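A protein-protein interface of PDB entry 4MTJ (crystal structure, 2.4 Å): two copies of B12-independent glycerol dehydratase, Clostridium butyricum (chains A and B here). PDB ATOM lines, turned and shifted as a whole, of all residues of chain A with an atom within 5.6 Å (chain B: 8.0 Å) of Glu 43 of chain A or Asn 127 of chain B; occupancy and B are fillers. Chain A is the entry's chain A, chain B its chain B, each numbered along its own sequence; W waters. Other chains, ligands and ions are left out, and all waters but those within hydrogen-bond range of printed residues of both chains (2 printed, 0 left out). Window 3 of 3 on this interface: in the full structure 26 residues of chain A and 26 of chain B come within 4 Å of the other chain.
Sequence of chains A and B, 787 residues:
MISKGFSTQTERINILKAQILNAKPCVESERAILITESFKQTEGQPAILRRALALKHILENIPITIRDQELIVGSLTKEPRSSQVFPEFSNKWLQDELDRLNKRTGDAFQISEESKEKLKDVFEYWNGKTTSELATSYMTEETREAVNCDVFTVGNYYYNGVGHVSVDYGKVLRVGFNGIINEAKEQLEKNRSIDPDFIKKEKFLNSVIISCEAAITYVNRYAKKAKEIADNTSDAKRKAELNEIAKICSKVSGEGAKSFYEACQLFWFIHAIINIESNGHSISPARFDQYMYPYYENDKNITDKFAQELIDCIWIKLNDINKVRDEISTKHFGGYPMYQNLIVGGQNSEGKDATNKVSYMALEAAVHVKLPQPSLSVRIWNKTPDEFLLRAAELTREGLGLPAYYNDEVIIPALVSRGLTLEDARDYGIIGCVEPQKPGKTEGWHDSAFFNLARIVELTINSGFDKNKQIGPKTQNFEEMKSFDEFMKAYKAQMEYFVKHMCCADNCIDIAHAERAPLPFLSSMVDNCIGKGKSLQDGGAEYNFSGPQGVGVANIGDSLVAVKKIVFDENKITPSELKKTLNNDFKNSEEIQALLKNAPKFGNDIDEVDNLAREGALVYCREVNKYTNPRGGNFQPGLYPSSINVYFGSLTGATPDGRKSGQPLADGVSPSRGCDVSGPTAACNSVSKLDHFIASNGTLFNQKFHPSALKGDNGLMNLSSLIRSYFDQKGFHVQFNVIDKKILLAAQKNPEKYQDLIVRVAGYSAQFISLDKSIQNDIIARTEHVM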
ATOM      1  N   PHE A  39     -35.069 -21.491 -14.101  1.00  0.00           N
ATOM      2  CA  PHE A  39     -35.022 -22.927 -13.821  1.00  0.00           C
ATOM      3  C   PHE A  39     -33.694 -23.366 -13.187  1.00  0.00           C
ATOM      4  O   PHE A  39     -33.672 -24.253 -12.333  1.00  0.00           O
ATOM      5  CB  PHE A  39     -35.328 -23.739 -15.084  1.00  0.00           C
ATOM      6  CG  PHE A  39     -36.739 -24.231 -15.147  1.00  0.00           C
ATOM      7  CD1 PHE A  39     -37.796 -23.332 -15.218  1.00  0.00           C
ATOM      8  CD2 PHE A  39     -37.015 -25.598 -15.120  1.00  0.00           C
ATOM      9  CE1 PHE A  39     -39.112 -23.783 -15.264  1.00  0.00           C
ATOM     10  CE2 PHE A  39     -38.319 -26.061 -15.156  1.00  0.00           C
ATOM     11  CZ  PHE A  39     -39.373 -25.151 -15.231  1.00  0.00           C
ATOM     12  N   LYS A  40     -32.598 -22.732 -13.598  1.00  0.00           N
ATOM     13  CA  LYS A  40     -31.284 -23.029 -13.034  1.00  0.00           C
ATOM     14  C   LYS A  40     -31.226 -22.709 -11.544  1.00  0.00           C
ATOM     15  O   LYS A  40     -30.430 -23.293 -10.809  1.00  0.00           O
ATOM     16  CB  LYS A  40     -30.196 -22.258 -13.774  1.00  0.00           C
ATOM     17  CG  LYS A  40     -29.891 -22.805 -15.158  1.00  0.00           C
ATOM     18  CD  LYS A  40     -28.939 -21.881 -15.892  1.00  0.00           C
ATOM     19  CE  LYS A  40     -28.455 -22.502 -17.193  1.00  0.00           C
ATOM     20  NZ  LYS A  40     -27.689 -21.510 -18.011  1.00  0.00           N
ATOM     21  N   GLN A  41     -32.083 -21.796 -11.105  1.00  0.00           N
ATOM     22  CA  GLN A  41     -32.116 -21.362  -9.709  1.00  0.00           C
ATOM     23  C   GLN A  41     -33.112 -22.121  -8.836  1.00  0.00           C
ATOM     24  O   GLN A  41     -33.171 -21.904  -7.619  1.00  0.00           O
ATOM     25  CB  GLN A  41     -32.433 -19.869  -9.643  1.00  0.00           C
ATOM     26  CG  GLN A  41     -31.359 -19.020 -10.277  1.00  0.00           C
ATOM     27  CD  GLN A  41     -30.011 -19.279  -9.643  1.00  0.00           C
ATOM     28  OE1 GLN A  41     -29.790 -18.922  -8.486  1.00  0.00           O
ATOM     29  NE2 GLN A  41     -29.108 -19.929 -10.384  1.00  0.00           N
ATOM     30  N   THR A  42     -33.892 -23.006  -9.451  1.00  0.00           N
ATOM     31  CA  THR A  42     -34.991 -23.651  -8.745  1.00  0.00           C
ATOM     32  C   THR A  42     -34.949 -25.177  -8.779  1.00  0.00           C
ATOM     33  O   THR A  42     -35.958 -25.827  -8.485  1.00  0.00           O
ATOM     34  CB  THR A  42     -36.362 -23.161  -9.273  1.00  0.00           C
ATOM     35  OG1 THR A  42     -36.498 -23.490 -10.664  1.00  0.00           O
ATOM     36  CG2 THR A  42     -36.488 -21.641  -9.094  1.00  0.00           C
ATOM     37  N   GLU A  43     -33.786 -25.744  -9.105  1.00  0.00           N
ATOM     38  CA  GLU A  43     -33.653 -27.192  -9.246  1.00  0.00           C
ATOM     39  C   GLU A  43     -34.179 -27.956  -8.027  1.00  0.00           C
ATOM     40  O   GLU A  43     -34.659 -29.082  -8.166  1.00  0.00           O
ATOM     41  CB  GLU A  43     -32.193 -27.597  -9.492  1.00  0.00           C
ATOM     42  CG  GLU A  43     -31.531 -26.943 -10.698  1.00  0.00           C
ATOM     43  CD  GLU A  43     -31.842 -27.635 -12.016  1.00  0.00           C
ATOM     44  OE1 GLU A  43     -32.599 -28.629 -12.030  1.00  0.00           O
ATOM     45  OE2 GLU A  43     -31.309 -27.174 -13.045  1.00  0.00           O
ATOM     46  N   GLY A  44     -34.089 -27.346  -6.843  1.00  0.00           N
ATOM     47  CA  GLY A  44     -34.470 -28.012  -5.611  1.00  0.00           C
ATOM     48  C   GLY A  44     -35.949 -27.912  -5.296  1.00  0.00           C
ATOM     49  O   GLY A  44     -36.413 -28.419  -4.282  1.00  0.00           O
ATOM     50  N   GLN A  45     -36.692 -27.278  -6.193  1.00  0.00           N
ATOM     51  CA  GLN A  45     -38.087 -26.950  -5.956  1.00  0.00           C
ATOM     52  C   GLN A  45     -39.014 -27.954  -6.673  1.00  0.00           C
ATOM     53  O   GLN A  45     -38.643 -28.500  -7.711  1.00  0.00           O
ATOM     54  CB  GLN A  45     -38.306 -25.530  -6.474  1.00  0.00           C
ATOM     55  CG  GLN A  45     -39.279 -24.710  -5.706  1.00  0.00           C
ATOM     56  CD  GLN A  45     -38.805 -24.340  -4.327  1.00  0.00           C
ATOM     57  OE1 GLN A  45     -39.454 -24.665  -3.329  1.00  0.00           O
ATOM     58  NE2 GLN A  45     -37.692 -23.627  -4.257  1.00  0.00           N
ATOM     59  N   ARG A  50     -41.416 -24.317  -9.492  1.00  0.00           N
ATOM     60  CA  ARG A  50     -40.531 -23.947 -10.597  1.00  0.00           C
ATOM     61  C   ARG A  50     -41.343 -23.141 -11.612  1.00  0.00           C
ATOM     62  O   ARG A  50     -40.906 -22.079 -12.069  1.00  0.00           O
ATOM     63  CB  ARG A  50     -39.923 -25.181 -11.278  1.00  0.00           C
ATOM     64  CG  ARG A  50     -39.095 -26.118 -10.380  1.00  0.00           C
ATOM     65  CD  ARG A  50     -37.654 -26.198 -10.872  1.00  0.00           C
ATOM     66  NE  ARG A  50     -37.373 -27.335 -11.726  1.00  0.00           N
ATOM     67  CZ  ARG A  50     -36.265 -27.476 -12.445  1.00  0.00           C
ATOM     68  NH1 ARG A  50     -35.336 -26.529 -12.436  1.00  0.00           N
ATOM     69  NH2 ARG A  50     -36.094 -28.562 -13.192  1.00  0.00           N
ATOM     70  N   TYR A 125     -29.122 -26.226 -21.824  1.00  0.00           N
ATOM     71  CA  TYR A 125     -29.720 -26.473 -20.514  1.00  0.00           C
ATOM     72  C   TYR A 125     -30.947 -27.399 -20.543  1.00  0.00           C
ATOM     73  O   TYR A 125     -31.107 -28.255 -19.670  1.00  0.00           O
ATOM     74  CB  TYR A 125     -30.106 -25.165 -19.800  1.00  0.00           C
ATOM     75  CG  TYR A 125     -30.890 -25.457 -18.533  1.00  0.00           C
ATOM     76  CD1 TYR A 125     -30.238 -25.864 -17.379  1.00  0.00           C
ATOM     77  CD2 TYR A 125     -32.285 -25.374 -18.511  1.00  0.00           C
ATOM     78  CE1 TYR A 125     -30.933 -26.167 -16.236  1.00  0.00           C
ATOM     79  CE2 TYR A 125     -32.993 -25.679 -17.367  1.00  0.00           C
ATOM     80  CZ  TYR A 125     -32.305 -26.077 -16.233  1.00  0.00           C
ATOM     81  OH  TYR A 125     -32.987 -26.385 -15.091  1.00  0.00           O
ATOM     82  N   LYS A 129     -34.867 -32.166 -20.493  1.00  0.00           N
ATOM     83  CA  LYS A 129     -35.666 -31.596 -19.409  1.00  0.00           C
ATOM     84  C   LYS A 129     -37.062 -31.136 -19.818  1.00  0.00           C
ATOM     85  O   LYS A 129     -37.794 -30.551 -19.006  1.00  0.00           O
ATOM     86  CB  LYS A 129     -34.903 -30.453 -18.719  1.00  0.00           C
ATOM     87  CG  LYS A 129     -33.556 -30.894 -18.135  1.00  0.00           C
ATOM     88  CD  LYS A 129     -32.879 -29.762 -17.365  1.00  0.00           C
ATOM     89  CE  LYS A 129     -31.467 -30.147 -16.957  1.00  0.00           C
ATOM     90  NZ  LYS A 129     -31.020 -29.327 -15.792  1.00  0.00           N
ATOM     91  N   GLU B  43     -31.708 -37.827 -18.217  1.00  0.00           N
ATOM     92  CA  GLU B  43     -32.438 -36.636 -17.859  1.00  0.00           C
ATOM     93  C   GLU B  43     -33.911 -36.689 -18.300  1.00  0.00           C
ATOM     94  O   GLU B  43     -34.793 -36.201 -17.585  1.00  0.00           O
ATOM     95  CB  GLU B  43     -31.722 -35.430 -18.465  1.00  0.00           C
ATOM     96  CG  GLU B  43     -31.731 -34.181 -17.606  1.00  0.00           C
ATOM     97  CD  GLU B  43     -30.891 -34.292 -16.345  1.00  0.00           C
ATOM     98  OE1 GLU B  43     -29.726 -34.749 -16.404  1.00  0.00           O
ATOM     99  OE2 GLU B  43     -31.405 -33.896 -15.286  1.00  0.00           O
ATOM    100  N   PRO B  87     -24.575 -39.390  -3.512  1.00  0.00           N
ATOM    101  CA  PRO B  87     -24.838 -37.950  -3.634  1.00  0.00           C
ATOM    102  C   PRO B  87     -26.280 -37.640  -3.988  1.00  0.00           C
ATOM    103  O   PRO B  87     -26.659 -36.466  -3.944  1.00  0.00           O
ATOM    104  CB  PRO B  87     -23.904 -37.515  -4.765  1.00  0.00           C
ATOM    105  CG  PRO B  87     -23.700 -38.764  -5.577  1.00  0.00           C
ATOM    106  CD  PRO B  87     -23.738 -39.902  -4.614  1.00  0.00           C
ATOM    107  N   ASN B  91     -24.930 -34.185  -0.402  1.00  0.00           N
ATOM    108  CA  ASN B  91     -23.503 -34.233  -0.699  1.00  0.00           C
ATOM    109  C   ASN B  91     -22.748 -32.977  -0.293  1.00  0.00           C
ATOM    110  O   ASN B  91     -21.522 -32.986  -0.211  1.00  0.00           O
ATOM    111  CB  ASN B  91     -23.278 -34.531  -2.187  1.00  0.00           C
ATOM    112  CG  ASN B  91     -23.973 -33.533  -3.085  1.00  0.00           C
ATOM    113  OD1 ASN B  91     -23.484 -32.414  -3.268  1.00  0.00           O
ATOM    114  ND2 ASN B  91     -25.125 -33.924  -3.644  1.00  0.00           N
ATOM    115  N   LYS B  92     -23.471 -31.894  -0.042  1.00  0.00           N
ATOM    116  CA  LYS B  92     -22.814 -30.647   0.339  1.00  0.00           C
ATOM    117  C   LYS B  92     -22.060 -30.767   1.668  1.00  0.00           C
ATOM    118  O   LYS B  92     -21.005 -30.147   1.842  1.00  0.00           O
ATOM    119  CB  LYS B  92     -23.802 -29.475   0.365  1.00  0.00           C
ATOM    120  CG  LYS B  92     -24.257 -28.998  -1.016  1.00  0.00           C
ATOM    121  CD  LYS B  92     -25.249 -27.843  -0.903  1.00  0.00           C
ATOM    122  CE  LYS B  92     -26.089 -27.676  -2.165  1.00  0.00           C
ATOM    123  NZ  LYS B  92     -25.234 -27.464  -3.357  1.00  0.00           N
ATOM    124  N   GLN B  95     -18.752 -32.169   0.764  1.00  0.00           N
ATOM    125  CA  GLN B  95     -17.928 -31.154   0.138  1.00  0.00           C
ATOM    126  C   GLN B  95     -17.348 -30.240   1.203  1.00  0.00           C
ATOM    127  O   GLN B  95     -16.227 -29.769   1.083  1.00  0.00           O
ATOM    128  CB  GLN B  95     -18.772 -30.340  -0.833  1.00  0.00           C
ATOM    129  CG  GLN B  95     -18.024 -29.229  -1.517  1.00  0.00           C
ATOM    130  CD  GLN B  95     -18.911 -28.461  -2.483  1.00  0.00           C
ATOM    131  OE1 GLN B  95     -20.063 -28.169  -2.179  1.00  0.00           O
ATOM    132  NE2 GLN B  95     -18.378 -28.143  -3.655  1.00  0.00           N
ATOM    133  N   ASP B 121     -16.878 -32.492  -9.674  1.00  0.00           N
ATOM    134  CA  ASP B 121     -17.919 -32.568 -10.696  1.00  0.00           C
ATOM    135  C   ASP B 121     -19.221 -33.165 -10.127  1.00  0.00           C
ATOM    136  O   ASP B 121     -20.319 -32.753 -10.498  1.00  0.00           O
ATOM    137  CB  ASP B 121     -17.433 -33.351 -11.917  1.00  0.00           C
ATOM    138  CG  ASP B 121     -18.534 -33.550 -12.966  1.00  0.00           C
ATOM    139  OD1 ASP B 121     -18.781 -34.719 -13.345  1.00  0.00           O
ATOM    140  OD2 ASP B 121     -19.154 -32.552 -13.409  1.00  0.00           O
ATOM    141  N   VAL B 122     -19.083 -34.117  -9.208  1.00  0.00           N
ATOM    142  CA  VAL B 122     -20.229 -34.686  -8.513  1.00  0.00           C
ATOM    143  C   VAL B 122     -21.013 -33.622  -7.730  1.00  0.00           C
ATOM    144  O   VAL B 122     -22.230 -33.530  -7.845  1.00  0.00           O
ATOM    145  CB  VAL B 122     -19.806 -35.835  -7.559  1.00  0.00           C
ATOM    146  CG1 VAL B 122     -21.003 -36.332  -6.760  1.00  0.00           C
ATOM    147  CG2 VAL B 122     -19.145 -36.975  -8.338  1.00  0.00           C
ATOM    148  N   PHE B 123     -20.308 -32.820  -6.938  1.00  0.00           N
ATOM    149  CA  PHE B 123     -20.949 -31.778  -6.145  1.00  0.00           C
ATOM    150  C   PHE B 123     -21.637 -30.798  -7.075  1.00  0.00           C
ATOM    151  O   PHE B 123     -22.737 -30.316  -6.788  1.00  0.00           O
ATOM    152  CB  PHE B 123     -19.918 -31.051  -5.264  1.00  0.00           C
ATOM    153  CG  PHE B 123     -19.237 -31.949  -4.266  1.00  0.00           C
ATOM    154  CD1 PHE B 123     -17.874 -31.863  -4.058  1.00  0.00           C
ATOM    155  CD2 PHE B 123     -19.969 -32.878  -3.536  1.00  0.00           C
ATOM    156  CE1 PHE B 123     -17.245 -32.691  -3.143  1.00  0.00           C
ATOM    157  CE2 PHE B 123     -19.350 -33.709  -2.625  1.00  0.00           C
ATOM    158  CZ  PHE B 123     -17.980 -33.621  -2.425  1.00  0.00           C
ATOM    159  N   GLU B 124     -20.985 -30.533  -8.204  1.00  0.00           N
ATOM    160  CA  GLU B 124     -21.497 -29.609  -9.209  1.00  0.00           C
ATOM    161  C   GLU B 124     -22.789 -30.102  -9.844  1.00  0.00           C
ATOM    162  O   GLU B 124     -23.789 -29.391  -9.854  1.00  0.00           O
ATOM    163  CB  GLU B 124     -20.452 -29.409 -10.298  1.00  0.00           C
ATOM    164  CG  GLU B 124     -20.679 -28.185 -11.150  1.00  0.00           C
ATOM    165  CD  GLU B 124     -19.403 -27.730 -11.832  1.00  0.00           C
ATOM    166  OE1 GLU B 124     -18.437 -27.387 -11.107  1.00  0.00           O
ATOM    167  OE2 GLU B 124     -19.362 -27.733 -13.084  1.00  0.00           O
ATOM    168  N   TYR B 125     -22.768 -31.323 -10.376  1.00  0.00           N
ATOM    169  CA  TYR B 125     -23.961 -31.865 -11.020  1.00  0.00           C
ATOM    170  C   TYR B 125     -25.177 -31.972 -10.101  1.00  0.00           C
ATOM    171  O   TYR B 125     -26.273 -31.591 -10.490  1.00  0.00           O
ATOM    172  CB  TYR B 125     -23.700 -33.237 -11.651  1.00  0.00           C
ATOM    173  CG  TYR B 125     -24.986 -33.817 -12.187  1.00  0.00           C
ATOM    174  CD1 TYR B 125     -25.542 -33.323 -13.356  1.00  0.00           C
ATOM    175  CD2 TYR B 125     -25.675 -34.818 -11.495  1.00  0.00           C
ATOM    176  CE1 TYR B 125     -26.720 -33.815 -13.842  1.00  0.00           C
ATOM    177  CE2 TYR B 125     -26.867 -35.317 -11.975  1.00  0.00           C
ATOM    178  CZ  TYR B 125     -27.387 -34.807 -13.151  1.00  0.00           C
ATOM    179  OH  TYR B 125     -28.571 -35.287 -13.661  1.00  0.00           O
ATOM    180  N   TRP B 126     -24.984 -32.498  -8.892  1.00  0.00           N
ATOM    181  CA  TRP B 126     -26.114 -32.808  -8.009  1.00  0.00           C
ATOM    182  C   TRP B 126     -26.732 -31.607  -7.292  1.00  0.00           C
ATOM    183  O   TRP B 126     -27.674 -31.765  -6.517  1.00  0.00           O
ATOM    184  CB  TRP B 126     -25.756 -33.914  -7.008  1.00  0.00           C
ATOM    185  CG  TRP B 126     -25.655 -35.256  -7.659  1.00  0.00           C
ATOM    186  CD1 TRP B 126     -24.520 -35.851  -8.145  1.00  0.00           C
ATOM    187  CD2 TRP B 126     -26.735 -36.165  -7.933  1.00  0.00           C
ATOM    188  NE1 TRP B 126     -24.827 -37.077  -8.685  1.00  0.00           N
ATOM    189  CE2 TRP B 126     -26.179 -37.293  -8.572  1.00  0.00           C
ATOM    190  CE3 TRP B 126     -28.115 -36.131  -7.706  1.00  0.00           C
ATOM    191  CZ2 TRP B 126     -26.956 -38.382  -8.980  1.00  0.00           C
ATOM    192  CZ3 TRP B 126     -28.882 -37.216  -8.104  1.00  0.00           C
ATOM    193  CH2 TRP B 126     -28.300 -38.328  -8.729  1.00  0.00           C
ATOM    194  N   ASN B 127     -26.210 -30.415  -7.571  1.00  0.00           N
ATOM    195  CA  ASN B 127     -26.717 -29.187  -6.971  1.00  0.00           C
ATOM    196  C   ASN B 127     -28.211 -28.998  -7.224  1.00  0.00           C
ATOM    197  O   ASN B 127     -28.643 -28.831  -8.365  1.00  0.00           O
ATOM    198  CB  ASN B 127     -25.939 -27.975  -7.491  1.00  0.00           C
ATOM    199  CG  ASN B 127     -26.242 -26.704  -6.704  1.00  0.00           C
ATOM    200  OD1 ASN B 127     -26.685 -26.752  -5.555  1.00  0.00           O
ATOM    201  ND2 ASN B 127     -26.008 -25.561  -7.324  1.00  0.00           N
ATOM    202  N   GLY B 128     -28.997 -29.030  -6.155  1.00  0.00           N
ATOM    203  CA  GLY B 128     -30.436 -28.877  -6.276  1.00  0.00           C
ATOM    204  C   GLY B 128     -31.197 -30.141  -6.642  1.00  0.00           C
ATOM    205  O   GLY B 128     -32.423 -30.141  -6.608  1.00  0.00           O
ATOM    206  N   LYS B 129     -30.480 -31.217  -6.966  1.00  0.00           N
ATOM    207  CA  LYS B 129     -31.108 -32.414  -7.533  1.00  0.00           C
ATOM    208  C   LYS B 129     -31.252 -33.594  -6.571  1.00  0.00           C
ATOM    209  O   LYS B 129     -31.589 -34.706  -6.993  1.00  0.00           O
ATOM    210  CB  LYS B 129     -30.351 -32.860  -8.784  1.00  0.00           C
ATOM    211  CG  LYS B 129     -30.215 -31.759  -9.820  1.00  0.00           C
ATOM    212  CD  LYS B 129     -29.400 -32.222 -11.009  1.00  0.00           C
ATOM    213  CE  LYS B 129     -29.333 -31.143 -12.090  1.00  0.00           C
ATOM    214  NZ  LYS B 129     -29.537 -31.756 -13.440  1.00  0.00           N
ATOM    215  N   THR B 130     -31.008 -33.353  -5.287  1.00  0.00           N
ATOM    216  CA  THR B 130     -31.024 -34.424  -4.301  1.00  0.00           C
ATOM    217  C   THR B 130     -32.392 -34.543  -3.638  1.00  0.00           C
ATOM    218  O   THR B 130     -33.233 -33.652  -3.757  1.00  0.00           O
ATOM    219  CB  THR B 130     -29.993 -34.182  -3.187  1.00  0.00           C
ATOM    220  OG1 THR B 130     -30.398 -33.056  -2.397  1.00  0.00           O
ATOM    221  CG2 THR B 130     -28.620 -33.929  -3.779  1.00  0.00           C
ATOM    222  N   GLU B 133     -32.728 -31.679  -0.854  1.00  0.00           N
ATOM    223  CA  GLU B 133     -33.076 -30.330  -1.299  1.00  0.00           C
ATOM    224  C   GLU B 133     -34.554 -30.205  -1.675  1.00  0.00           C
ATOM    225  O   GLU B 133     -35.177 -29.144  -1.470  1.00  0.00           O
ATOM    226  CB  GLU B 133     -32.169 -29.895  -2.449  1.00  0.00           C
ATOM    227  CG  GLU B 133     -30.720 -29.699  -2.017  1.00  0.00           C
ATOM    228  CD  GLU B 133     -29.734 -29.880  -3.153  1.00  0.00           C
ATOM    229  OE1 GLU B 133     -28.954 -28.938  -3.419  1.00  0.00           O
ATOM    230  OE2 GLU B 133     -29.744 -30.962  -3.781  1.00  0.00           O
ATOM    231  N   LEU B 134     -35.121 -31.279  -2.215  1.00  0.00           N
ATOM    232  CA  LEU B 134     -36.561 -31.292  -2.480  1.00  0.00           C
ATOM    233  C   LEU B 134     -37.346 -31.345  -1.154  1.00  0.00           C
ATOM    234  O   LEU B 134     -38.364 -30.667  -0.988  1.00  0.00           O
ATOM    235  CB  LEU B 134     -36.930 -32.469  -3.385  1.00  0.00           C
ATOM    236  CG  LEU B 134     -38.420 -32.615  -3.677  1.00  0.00           C
ATOM    237  CD1 LEU B 134     -38.935 -31.398  -4.423  1.00  0.00           C
ATOM    238  CD2 LEU B 134     -38.654 -33.880  -4.459  1.00  0.00           C
ATOM    239  N   SER B 137     -37.610 -28.049   0.389  1.00  0.00           N
ATOM    240  CA  SER B 137     -38.584 -27.291  -0.409  1.00  0.00           C
ATOM    241  C   SER B 137     -40.038 -27.582  -0.023  1.00  0.00           C
ATOM    242  O   SER B 137     -40.873 -26.681   0.009  1.00  0.00           O
ATOM    243  CB  SER B 137     -38.401 -27.567  -1.902  1.00  0.00           C
ATOM    244  OG  SER B 137     -37.224 -26.970  -2.399  1.00  0.00           O
ATOM    245  N   ARG B 516     -37.903 -38.470  -6.032  1.00  0.00           N
ATOM    246  CA  ARG B 516     -36.582 -38.456  -6.667  1.00  0.00           C
ATOM    247  C   ARG B 516     -35.794 -39.742  -6.494  1.00  0.00           C
ATOM    248  O   ARG B 516     -34.844 -39.978  -7.219  1.00  0.00           O
ATOM    249  CB  ARG B 516     -35.746 -37.273  -6.178  1.00  0.00           C
ATOM    250  CG  ARG B 516     -36.341 -35.922  -6.555  1.00  0.00           C
ATOM    251  CD  ARG B 516     -35.434 -34.752  -6.178  1.00  0.00           C
ATOM    252  NE  ARG B 516     -35.893 -33.531  -6.830  1.00  0.00           N
ATOM    253  CZ  ARG B 516     -35.255 -32.364  -6.785  1.00  0.00           C
ATOM    254  NH1 ARG B 516     -34.118 -32.235  -6.106  1.00  0.00           N
ATOM    255  NH2 ARG B 516     -35.753 -31.322  -7.425  1.00  0.00           N
HETATM  256  O   HOH W   1     -40.108 -23.900  -0.892  1.00  0.00           O
HETATM  257  O   HOH W   2     -38.404 -30.669  -9.230  1.00  0.00           O
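Glu 43 of chain A touches just these residues of chain B: Asn 127, Gly 128 and Arg 516. Asn 127 of chain B touches just one residue of chain A: Glu 43. Of the printed residues of chain B, Lys 129 of chain A touches Glu 43 and Lys 129. Printed residues of chain B within 4 Å of Gln 45 of chain A: Ser 137 (3.3 Å). Asp 121 of chain B touches none of the printed residues of chain A. The nearest residue of chain B that does not touch Glu 43 of chain A is Lys 129 of chain B (4.1 Å).
The backbone carbonyl oxygen of Gly 44 of chain A sits close to the backbone carbonyl oxygen of Glu 133 of chain B (3.2 Å). The side-chain hydroxyl (OG) of Ser 137 of chain B is in hydrogen-bond range of the side-chain amide oxygen (OE1) of Gln 45 of chain A, at 3.3 Å. N of Gly 44 of chain A sits close to O of Gly 128 of chain B, 3.3 Å away. O of Glu 43 of chain A lies close to O of Gly 128 of chain B (2.9 Å). The backbone carbonyl oxygen (O) of Glu 43 of chain A sits at hydrogen-bond distance from the guanidinium group (NH2) of Arg 516 of chain B (2.6 Å). OG of Ser 137 of chain B lies within hydrogen-bond range of O of Gly 44 of chain A, at 2.5 Å.
Glu 43 of chain A touches Asn 127 of chain B (CB to O, 3.9 Å). Gly 44 of chain A touches Leu 134 of chain B (O to CA, 3.4 Å). CA of Gly 44 of chain A touches NH2 of Arg 516 of chain B, 3.99 Å away. Glu 43 of chain B touches Lys 129 of chain A. Lys 129 of chain B touches Lys 129 of chain A (NZ to NZ, 3.7 Å).
The side-chain amino group (NZ) of Lys 92 of chain B lies within hydrogen-bond range of the side-chain amide oxygen (OD1) of Asn 127 of chain B (2.7 Å). OH of Tyr 125 of chain B lies within hydrogen-bond range of OE1 of Glu 43 of chain B, 3.0 Å away. The side-chain carboxylate (OE2) of Glu 133 of chain B lies within hydrogen-bond range of the side-chain hydroxyl (OG1) of Thr 130 of chain B (2.6 Å). The backbone carbonyl oxygen (O) of Glu 133 of chain B is in hydrogen-bond range of the side-chain hydroxyl (OG) of Ser 137 of chain B (3.1 Å). N of Lys 129 of chain B sits at hydrogen-bond distance from OE2 of Glu 133 of chain B, 3.3 Å away. The side-chain carboxylate (OE2) of Glu 43 of chain A sits at hydrogen-bond distance from the side-chain hydroxyl (OH) of Tyr 125 of chain A (2.8 Å).
Printed residues of chain A that touch a printed residue of chain B: Glu 43, Gly 44, Gln 45 and Lys 129. Of the 19 printed residues of chain B, 8 touch a printed residue of chain A. Printed residues of chain B that touch a printed residue of chain A: Glu 43, Asn 127, Gly 128, Lys 129, Glu 133, Leu 134, Ser 137 and Arg 516.
Lys 129 of chain A touches Glu 43 of chain B, but with the chains exchanged Glu 43 of chain A does not touch Lys 129 of chain B (4.1 Å). Lys 129 of chain A touches its own counterpart, Lys 129 of chain B. 3 positions are printed for both chains. Of the 11 pairs that touch across the chains among the printed residues, 1 has its exchanged pair printed and touching as well.
Water W1 lies within hydrogen-bond range of OE1 of Gln 45 of chain A (2.6 Å) and O of Ser 137 of chain B (3.0 Å). Water W2 bridges the backbone carbonyl oxygen of Gln 45 of chain A (2.7 Å) and the guanidinium group of Arg 516 of chain B (3.3 Å).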
